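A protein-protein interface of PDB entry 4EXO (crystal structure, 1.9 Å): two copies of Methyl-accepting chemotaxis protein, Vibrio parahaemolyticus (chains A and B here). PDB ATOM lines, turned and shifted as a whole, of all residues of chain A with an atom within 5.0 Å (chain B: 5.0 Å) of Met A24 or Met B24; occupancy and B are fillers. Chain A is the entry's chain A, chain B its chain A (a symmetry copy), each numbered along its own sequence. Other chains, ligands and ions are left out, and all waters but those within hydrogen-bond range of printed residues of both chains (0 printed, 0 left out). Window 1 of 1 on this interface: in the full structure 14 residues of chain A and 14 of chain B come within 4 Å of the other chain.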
ATOM      1  N   ALA A  20      25.180  18.027  13.534  1.00  0.00           N
ATOM      2  CA  ALA A  20      24.988  17.166  14.717  1.00  0.00           C
ATOM      3  C   ALA A  20      23.643  16.450  14.689  1.00  0.00           C
ATOM      4  O   ALA A  20      23.559  15.235  14.912  1.00  0.00           O
ATOM      5  CB  ALA A  20      25.110  17.993  16.033  1.00  0.00           C
ATOM      6  N   TYR A  21      22.576  17.199  14.445  1.00  0.00           N
ATOM      7  CA  TYR A  21      21.242  16.579  14.390  1.00  0.00           C
ATOM      8  C   TYR A  21      21.187  15.543  13.289  1.00  0.00           C
ATOM      9  O   TYR A  21      20.604  14.474  13.484  1.00  0.00           O
ATOM     10  CB  TYR A  21      20.170  17.648  14.103  1.00  0.00           C
ATOM     11  CG  TYR A  21      20.088  18.755  15.176  1.00  0.00           C
ATOM     12  CD1 TYR A  21      20.296  18.457  16.517  1.00  0.00           C
ATOM     13  CD2 TYR A  21      19.774  20.069  14.825  1.00  0.00           C
ATOM     14  CE1 TYR A  21      20.198  19.430  17.504  1.00  0.00           C
ATOM     15  CE2 TYR A  21      19.669  21.061  15.800  1.00  0.00           C
ATOM     16  CZ  TYR A  21      19.879  20.732  17.127  1.00  0.00           C
ATOM     17  OH  TYR A  21      19.808  21.705  18.096  1.00  0.00           O
ATOM     18  N   MET A  22      21.776  15.865  12.120  1.00  0.00           N
ATOM     19  CA  MET A  22      21.793  14.896  11.028  1.00  0.00           C
ATOM     20  C   MET A  22      22.538  13.621  11.464  1.00  0.00           C
ATOM     21  O   MET A  22      22.077  12.509  11.191  1.00  0.00           O
ATOM     22  CB  MET A  22      22.446  15.472   9.746  1.00  0.00           C
ATOM     23  CG  MET A  22      22.501  14.468   8.565  1.00  0.00           C
ATOM     24  SD  MET A  22      20.740  13.758   7.998  1.00  0.00           S
ATOM     25  CE  MET A  22      19.850  15.452   7.784  1.00  0.00           C
ATOM     26  N   MET A  23      23.692  13.783  12.104  1.00  0.00           N
ATOM     27  CA  MET A  23      24.438  12.635  12.623  1.00  0.00           C
ATOM     28  C   MET A  23      23.587  11.764  13.529  1.00  0.00           C
ATOM     29  O   MET A  23      23.621  10.544  13.432  1.00  0.00           O
ATOM     30  CB  MET A  23      25.710  13.051  13.376  1.00  0.00           C
ATOM     31  CG  MET A  23      26.544  11.844  13.692  1.00  0.00           C
ATOM     32  SD  MET A  23      28.214  12.368  14.574  1.00  0.00           S
ATOM     33  CE  MET A  23      29.256  13.061  13.092  1.00  0.00           C
ATOM     34  N   MET A  24      22.786  12.386  14.387  1.00  0.00           N
ATOM     35  CA  MET A  24      21.919  11.609  15.273  1.00  0.00           C
ATOM     36  C   MET A  24      20.907  10.761  14.526  1.00  0.00           C
ATOM     37  O   MET A  24      20.670   9.610  14.894  1.00  0.00           O
ATOM     38  CB  MET A  24      21.220  12.525  16.276  1.00  0.00           C
ATOM     39  CG  MET A  24      22.213  13.256  17.144  1.00  0.00           C
ATOM     40  SD  MET A  24      21.347  14.146  18.628  1.00  0.00           S
ATOM     41  CE  MET A  24      20.730  12.628  19.649  1.00  0.00           C
ATOM     42  N   GLY A  25      20.304  11.334  13.486  1.00  0.00           N
ATOM     43  CA  GLY A  25      19.327  10.609  12.694  1.00  0.00           C
ATOM     44  C   GLY A  25      19.974   9.442  11.928  1.00  0.00           C
ATOM     45  O   GLY A  25      19.487   8.322  11.974  1.00  0.00           O
ATOM     46  N   VAL A  26      21.099   9.726  11.272  1.00  0.00           N
ATOM     47  CA  VAL A  26      21.851   8.742  10.526  1.00  0.00           C
ATOM     48  C   VAL A  26      22.345   7.591  11.434  1.00  0.00           C
ATOM     49  O   VAL A  26      22.264   6.404  11.061  1.00  0.00           O
ATOM     50  CB  VAL A  26      23.015   9.420   9.719  1.00  0.00           C
ATOM     51  CG1 VAL A  26      23.979   8.354   9.082  1.00  0.00           C
ATOM     52  CG2 VAL A  26      22.412  10.345   8.606  1.00  0.00           C
ATOM     53  N   THR A  27      22.813   7.931  12.621  1.00  0.00           N
ATOM     54  CA  THR A  27      23.299   6.887  13.526  1.00  0.00           C
ATOM     55  C   THR A  27      22.150   6.143  14.224  1.00  0.00           C
ATOM     56  O   THR A  27      22.273   4.954  14.464  1.00  0.00           O
ATOM     57  CB  THR A  27      24.340   7.427  14.533  1.00  0.00           C
ATOM     58  OG1 THR A  27      23.789   8.524  15.263  1.00  0.00           O
ATOM     59  CG2 THR A  27      25.590   7.923  13.779  1.00  0.00           C
ATOM     60  N   ALA A  28      21.028   6.814  14.492  1.00  0.00           N
ATOM     61  CA  ALA A  28      19.868   6.132  15.073  1.00  0.00           C
ATOM     62  C   ALA A  28      19.382   4.962  14.219  1.00  0.00           C
ATOM     63  O   ALA A  28      18.905   3.956  14.774  1.00  0.00           O
ATOM     64  CB  ALA A  28      18.711   7.111  15.366  1.00  0.00           C
ATOM     65  N   MET A  52      11.432  11.398  15.548  1.00  0.00           N
ATOM     66  CA  MET A  52      12.459  12.273  16.121  1.00  0.00           C
ATOM     67  C   MET A  52      12.206  13.783  16.029  1.00  0.00           C
ATOM     68  O   MET A  52      11.766  14.316  14.981  1.00  0.00           O
ATOM     69  CB  MET A  52      13.847  11.953  15.511  1.00  0.00           C
ATOM     70  CG  MET A  52      14.342  10.597  15.974  1.00  0.00           C
ATOM     71  SD  MET A  52      15.918   9.980  15.017  1.00  0.00           S
ATOM     72  CE  MET A  52      17.132  11.117  15.903  1.00  0.00           C
ATOM     73  N   ARG A  53      12.493  14.475  17.132  1.00  0.00           N
ATOM     74  CA  ARG A  53      12.449  15.951  17.140  1.00  0.00           C
ATOM     75  C   ARG A  53      13.618  16.508  17.919  1.00  0.00           C
ATOM     76  O   ARG A  53      13.980  15.939  18.960  1.00  0.00           O
ATOM     77  CB  ARG A  53      11.151  16.455  17.820  1.00  0.00           C
ATOM     78  CG  ARG A  53       9.870  15.975  17.155  1.00  0.00           C
ATOM     79  CD  ARG A  53       9.578  16.783  15.861  1.00  0.00           C
ATOM     80  NE  ARG A  53       8.247  16.434  15.338  1.00  0.00           N
ATOM     81  CZ  ARG A  53       7.955  15.282  14.737  1.00  0.00           C
ATOM     82  NH1 ARG A  53       8.906  14.353  14.535  1.00  0.00           N
ATOM     83  NH2 ARG A  53       6.713  15.075  14.285  1.00  0.00           N
ATOM     84  N   PHE A  54      14.196  17.622  17.455  1.00  0.00           N
ATOM     85  CA  PHE A  54      15.089  18.395  18.324  1.00  0.00           C
ATOM     86  C   PHE A  54      14.446  19.684  18.874  1.00  0.00           C
ATOM     87  O   PHE A  54      15.049  20.385  19.698  1.00  0.00           O
ATOM     88  CB  PHE A  54      16.455  18.673  17.657  1.00  0.00           C
ATOM     89  CG  PHE A  54      16.373  19.384  16.298  1.00  0.00           C
ATOM     90  CD1 PHE A  54      16.342  20.775  16.224  1.00  0.00           C
ATOM     91  CD2 PHE A  54      16.347  18.660  15.121  1.00  0.00           C
ATOM     92  CE1 PHE A  54      16.281  21.448  14.955  1.00  0.00           C
ATOM     93  CE2 PHE A  54      16.293  19.333  13.836  1.00  0.00           C
ATOM     94  CZ  PHE A  54      16.259  20.717  13.780  1.00  0.00           C
ATOM     95  N   PHE A  60      12.680  15.472  10.523  1.00  0.00           N
ATOM     96  CA  PHE A  60      13.255  14.915   9.294  1.00  0.00           C
ATOM     97  C   PHE A  60      12.261  14.731   8.148  1.00  0.00           C
ATOM     98  O   PHE A  60      11.052  14.466   8.373  1.00  0.00           O
ATOM     99  CB  PHE A  60      13.867  13.542   9.569  1.00  0.00           C
ATOM    100  CG  PHE A  60      15.098  13.589  10.400  1.00  0.00           C
ATOM    101  CD1 PHE A  60      16.326  13.935   9.831  1.00  0.00           C
ATOM    102  CD2 PHE A  60      15.038  13.270  11.753  1.00  0.00           C
ATOM    103  CE1 PHE A  60      17.494  13.971  10.592  1.00  0.00           C
ATOM    104  CE2 PHE A  60      16.211  13.297  12.557  1.00  0.00           C
ATOM    105  CZ  PHE A  60      17.446  13.663  11.980  1.00  0.00           C
ATOM    106  N   ALA B  20      18.372  19.574  23.478  1.00  0.00           N
ATOM    107  CA  ALA B  20      18.007  19.145  22.113  1.00  0.00           C
ATOM    108  C   ALA B  20      18.418  17.705  21.839  1.00  0.00           C
ATOM    109  O   ALA B  20      17.629  16.898  21.332  1.00  0.00           O
ATOM    110  CB  ALA B  20      18.648  20.083  21.045  1.00  0.00           C
ATOM    111  N   TYR B  21      19.667  17.376  22.142  1.00  0.00           N
ATOM    112  CA  TYR B  21      20.139  15.999  21.916  1.00  0.00           C
ATOM    113  C   TYR B  21      19.323  15.023  22.735  1.00  0.00           C
ATOM    114  O   TYR B  21      18.979  13.948  22.239  1.00  0.00           O
ATOM    115  CB  TYR B  21      21.615  15.867  22.335  1.00  0.00           C
ATOM    116  CG  TYR B  21      22.574  16.786  21.547  1.00  0.00           C
ATOM    117  CD1 TYR B  21      22.350  17.051  20.201  1.00  0.00           C
ATOM    118  CD2 TYR B  21      23.696  17.343  22.161  1.00  0.00           C
ATOM    119  CE1 TYR B  21      23.215  17.850  19.463  1.00  0.00           C
ATOM    120  CE2 TYR B  21      24.578  18.147  21.437  1.00  0.00           C
ATOM    121  CZ  TYR B  21      24.331  18.390  20.098  1.00  0.00           C
ATOM    122  OH  TYR B  21      25.174  19.205  19.380  1.00  0.00           O
ATOM    123  N   MET B  22      19.031  15.384  24.000  1.00  0.00           N
ATOM    124  CA  MET B  22      18.215  14.505  24.832  1.00  0.00           C
ATOM    125  C   MET B  22      16.831  14.302  24.188  1.00  0.00           C
ATOM    126  O   MET B  22      16.323  13.178  24.148  1.00  0.00           O
ATOM    127  CB  MET B  22      18.046  15.054  26.272  1.00  0.00           C
ATOM    128  CG  MET B  22      17.171  14.158  27.186  1.00  0.00           C
ATOM    129  SD  MET B  22      17.820  12.298  27.393  1.00  0.00           S
ATOM    130  CE  MET B  22      19.628  12.723  27.904  1.00  0.00           C
ATOM    131  N   MET B  23      16.213  15.385  23.724  1.00  0.00           N
ATOM    132  CA  MET B  23      14.929  15.285  23.030  1.00  0.00           C
ATOM    133  C   MET B  23      14.983  14.314  21.866  1.00  0.00           C
ATOM    134  O   MET B  23      14.075  13.513  21.678  1.00  0.00           O
ATOM    135  CB  MET B  23      14.425  16.646  22.526  1.00  0.00           C
ATOM    136  CG  MET B  23      13.016  16.523  22.024  1.00  0.00           C
ATOM    137  SD  MET B  23      12.327  18.270  21.460  1.00  0.00           S
ATOM    138  CE  MET B  23      11.955  19.128  23.160  1.00  0.00           C
ATOM    139  N   MET B  24      16.067  14.348  21.099  1.00  0.00           N
ATOM    140  CA  MET B  24      16.198  13.422  19.974  1.00  0.00           C
ATOM    141  C   MET B  24      16.214  11.966  20.398  1.00  0.00           C
ATOM    142  O   MET B  24      15.589  11.125  19.750  1.00  0.00           O
ATOM    143  CB  MET B  24      17.438  13.757  19.147  1.00  0.00           C
ATOM    144  CG  MET B  24      17.365  15.151  18.577  1.00  0.00           C
ATOM    145  SD  MET B  24      18.749  15.461  17.261  1.00  0.00           S
ATOM    146  CE  MET B  24      18.189  14.258  15.859  1.00  0.00           C
ATOM    147  N   GLY B  25      16.937  11.668  21.476  1.00  0.00           N
ATOM    148  CA  GLY B  25      17.011  10.307  21.975  1.00  0.00           C
ATOM    149  C   GLY B  25      15.652   9.825  22.509  1.00  0.00           C
ATOM    150  O   GLY B  25      15.189   8.751  22.156  1.00  0.00           O
ATOM    151  N   VAL B  26      15.012  10.665  23.324  1.00  0.00           N
ATOM    152  CA  VAL B  26      13.713  10.383  23.892  1.00  0.00           C
ATOM    153  C   VAL B  26      12.638  10.193  22.796  1.00  0.00           C
ATOM    154  O   VAL B  26      11.806   9.267  22.872  1.00  0.00           O
ATOM    155  CB  VAL B  26      13.315  11.476  24.947  1.00  0.00           C
ATOM    156  CG1 VAL B  26      11.821  11.317  25.413  1.00  0.00           C
ATOM    157  CG2 VAL B  26      14.281  11.394  26.179  1.00  0.00           C
ATOM    158  N   THR B  27      12.678  11.028  21.774  1.00  0.00           N
ATOM    159  CA  THR B  27      11.686  10.900  20.704  1.00  0.00           C
ATOM    160  C   THR B  27      12.017   9.749  19.740  1.00  0.00           C
ATOM    161  O   THR B  27      11.103   9.112  19.243  1.00  0.00           O
ATOM    162  CB  THR B  27      11.456  12.236  19.960  1.00  0.00           C
ATOM    163  OG1 THR B  27      12.697  12.731  19.453  1.00  0.00           O
ATOM    164  CG2 THR B  27      10.873  13.282  20.931  1.00  0.00           C
ATOM    165  N   ALA B  28      13.298   9.449  19.525  1.00  0.00           N
ATOM    166  CA  ALA B  28      13.669   8.304  18.686  1.00  0.00           C
ATOM    167  C   ALA B  28      13.080   6.989  19.191  1.00  0.00           C
ATOM    168  O   ALA B  28      12.745   6.114  18.372  1.00  0.00           O
ATOM    169  CB  ALA B  28      15.198   8.187  18.515  1.00  0.00           C
ATOM    170  N   MET B  52      23.313   5.833  18.604  1.00  0.00           N
ATOM    171  CA  MET B  52      23.288   7.277  18.357  1.00  0.00           C
ATOM    172  C   MET B  52      24.536   8.067  18.771  1.00  0.00           C
ATOM    173  O   MET B  52      25.116   7.859  19.866  1.00  0.00           O
ATOM    174  CB  MET B  52      22.039   7.920  19.012  1.00  0.00           C
ATOM    175  CG  MET B  52      20.773   7.490  18.298  1.00  0.00           C
ATOM    176  SD  MET B  52      19.146   7.991  19.239  1.00  0.00           S
ATOM    177  CE  MET B  52      19.213   9.815  18.769  1.00  0.00           C
ATOM    178  N   ARG B  53      24.945   8.985  17.894  1.00  0.00           N
ATOM    179  CA  ARG B  53      26.034   9.925  18.226  1.00  0.00           C
ATOM    180  C   ARG B  53      25.705  11.311  17.719  1.00  0.00           C
ATOM    181  O   ARG B  53      25.152  11.438  16.616  1.00  0.00           O
ATOM    182  CB  ARG B  53      27.358   9.485  17.555  1.00  0.00           C
ATOM    183  CG  ARG B  53      27.832   8.096  17.958  1.00  0.00           C
ATOM    184  CD  ARG B  53      28.483   8.117  19.368  1.00  0.00           C
ATOM    185  NE  ARG B  53      29.098   6.812  19.659  1.00  0.00           N
ATOM    186  CZ  ARG B  53      28.414   5.706  19.942  1.00  0.00           C
ATOM    187  NH1 ARG B  53      27.072   5.730  20.017  1.00  0.00           N
ATOM    188  NH2 ARG B  53      29.077   4.575  20.206  1.00  0.00           N
ATOM    189  N   PHE B  54      26.057  12.349  18.486  1.00  0.00           N
ATOM    190  CA  PHE B  54      26.082  13.700  17.915  1.00  0.00           C
ATOM    191  C   PHE B  54      27.504  14.215  17.618  1.00  0.00           C
ATOM    192  O   PHE B  54      27.674  15.299  17.045  1.00  0.00           O
ATOM    193  CB  PHE B  54      25.271  14.706  18.762  1.00  0.00           C
ATOM    194  CG  PHE B  54      25.701  14.798  20.234  1.00  0.00           C
ATOM    195  CD1 PHE B  54      26.712  15.674  20.626  1.00  0.00           C
ATOM    196  CD2 PHE B  54      25.081  14.030  21.201  1.00  0.00           C
ATOM    197  CE1 PHE B  54      27.108  15.777  22.004  1.00  0.00           C
ATOM    198  CE2 PHE B  54      25.471  14.135  22.596  1.00  0.00           C
ATOM    199  CZ  PHE B  54      26.482  15.007  22.968  1.00  0.00           C
ATOM    200  N   PHE B  60      24.865   8.236  24.538  1.00  0.00           N
ATOM    201  CA  PHE B  60      23.945   7.996  25.656  1.00  0.00           C
ATOM    202  C   PHE B  60      24.384   6.896  26.621  1.00  0.00           C
ATOM    203  O   PHE B  60      25.052   5.908  26.221  1.00  0.00           O
ATOM    204  CB  PHE B  60      22.566   7.596  25.132  1.00  0.00           C
ATOM    205  CG  PHE B  60      21.835   8.702  24.462  1.00  0.00           C
ATOM    206  CD1 PHE B  60      21.178   9.677  25.217  1.00  0.00           C
ATOM    207  CD2 PHE B  60      21.784   8.764  23.073  1.00  0.00           C
ATOM    208  CE1 PHE B  60      20.474  10.715  24.607  1.00  0.00           C
ATOM    209  CE2 PHE B  60      21.075   9.810  22.419  1.00  0.00           C
ATOM    210  CZ  PHE B  60      20.426  10.801  23.187  1.00  0.00           C
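The backbone carbonyl oxygen of Arg A53 lies within hydrogen-bond range of the backbone NH of Met B24 (3.4 Å).
The side-chain hydroxyl of Thr A27 sits at hydrogen-bond distance from the backbone NH of Arg B53 (2.9 Å).
The backbone NH (N) of Arg A53 lies within hydrogen-bond range of the side-chain hydroxyl (OG1) of Thr B27, at 2.9 Å.
The side-chain sulfur of Met A23 lies close to the backbone carbonyl oxygen of Arg B53 (3.8 Å).
The side-chain sulfur of Met A24 sits close to the side-chain sulfur of Met B24 (3.2 Å).
The backbone carbonyl oxygen of Arg A53 lies close to the side-chain sulfur of Met B23 (3.8 Å).
The backbone NH (N) of Met A24 sits at hydrogen-bond distance from the backbone carbonyl oxygen (O) of Arg B53.
O of Met B24 is in hydrogen-bond range of OG1 of Thr B27 (3.3 Å).
The backbone carbonyl oxygen of Met A23 is in hydrogen-bond range of the side-chain hydroxyl of Thr A27, 2.7 Å away.
The backbone carbonyl oxygen of Met A24 is in hydrogen-bond range of the side-chain hydroxyl of Thr A27 (3.3 Å).
O of Met B23 lies within hydrogen-bond range of OG1 of Thr B27 (2.7 Å).
Among the printed residues, pairs that only touch across the chains: Ala A20 with Tyr B21, Ala A20 with Phe B54, Tyr A21 with Ala B20, Tyr A21 with Tyr B21, Tyr A21 with Met B24, Met A23 with Phe B54, Met A24 with Tyr B21, Met A24 with Met B52, Met A24 with Phe B54, Met A24 with Phe B60, Thr A27 with Met B52, Ala A28 with Met B52, Met A52 with Met B24, Met A52 with Thr B27, Met A52 with Ala B28, Met A52 with Met B52, Phe A54 with Ala B20, Phe A54 with Met B23, Phe A54 with Met B24 and Phe A60 with Met B24.
Of the printed residues of chain B, Met A23 touches Arg B53 and Phe B54.
Of the printed residues of chain B, Met A24 touches Tyr B21 (3.4 Å), Met B24 (3.2 Å), Met B52 (3.3 Å), Arg B53 (3.4 Å), Phe B54 (3.8 Å) and Phe B60 (3.97 Å).
Printed residues of chain A within 4 Å of Ala B20: Tyr A21 (3.6 Å) and Phe A54 (3.9 Å).
Of the printed residues of chain A, Met B24 touches Tyr A21, Met A24, Met A52, Arg A53, Phe A54 and Phe A60.
Of the printed residues of chain A, Arg B53 touches Met A23, Met A24 and Thr A27.
The nearest printed residue of chain A that does not touch Met B24 is Gly A25 (4.3 Å).
Hydrophobic or aromatic side chains of chain B that line the printed part of chain A: Ala B20, Tyr B21, Met B23, Met B24, Ala B28, Met B52, Phe B54 and Phe B60.
Of the 13 printed residues of chain A, 10 touch a printed residue of chain B.
Printed residues of chain A that touch a printed residue of chain B: Ala A20, Tyr A21, Met A23, Met A24, Thr A27, Ala A28, Met A52, Arg A53, Phe A54 and Phe A60.
Hydrophobic or aromatic side chains of chain A within 4 Å of the printed part of chain B: Ala A20, Tyr A21, Met A23, Met A24, Ala A28, Met A52, Phe A54 and Phe A60.
Among the printed residues, 27 pairs touch across the chains.
Among the printed residues, no Asp or Glu carboxylate lies within 4 Å of a Lys or Arg side-chain nitrogen of the other chain.
Ala A20 touches Phe B54, and with the chains exchanged Phe A54 touches Ala B20.
Tyr B21 touches its own counterpart, Tyr A21.
Met A23 touches Phe B54, and with the chains exchanged Phe A54 touches Met B23.
Met A24 touches Met B52, and with the chains exchanged Met A52 touches Met B24.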
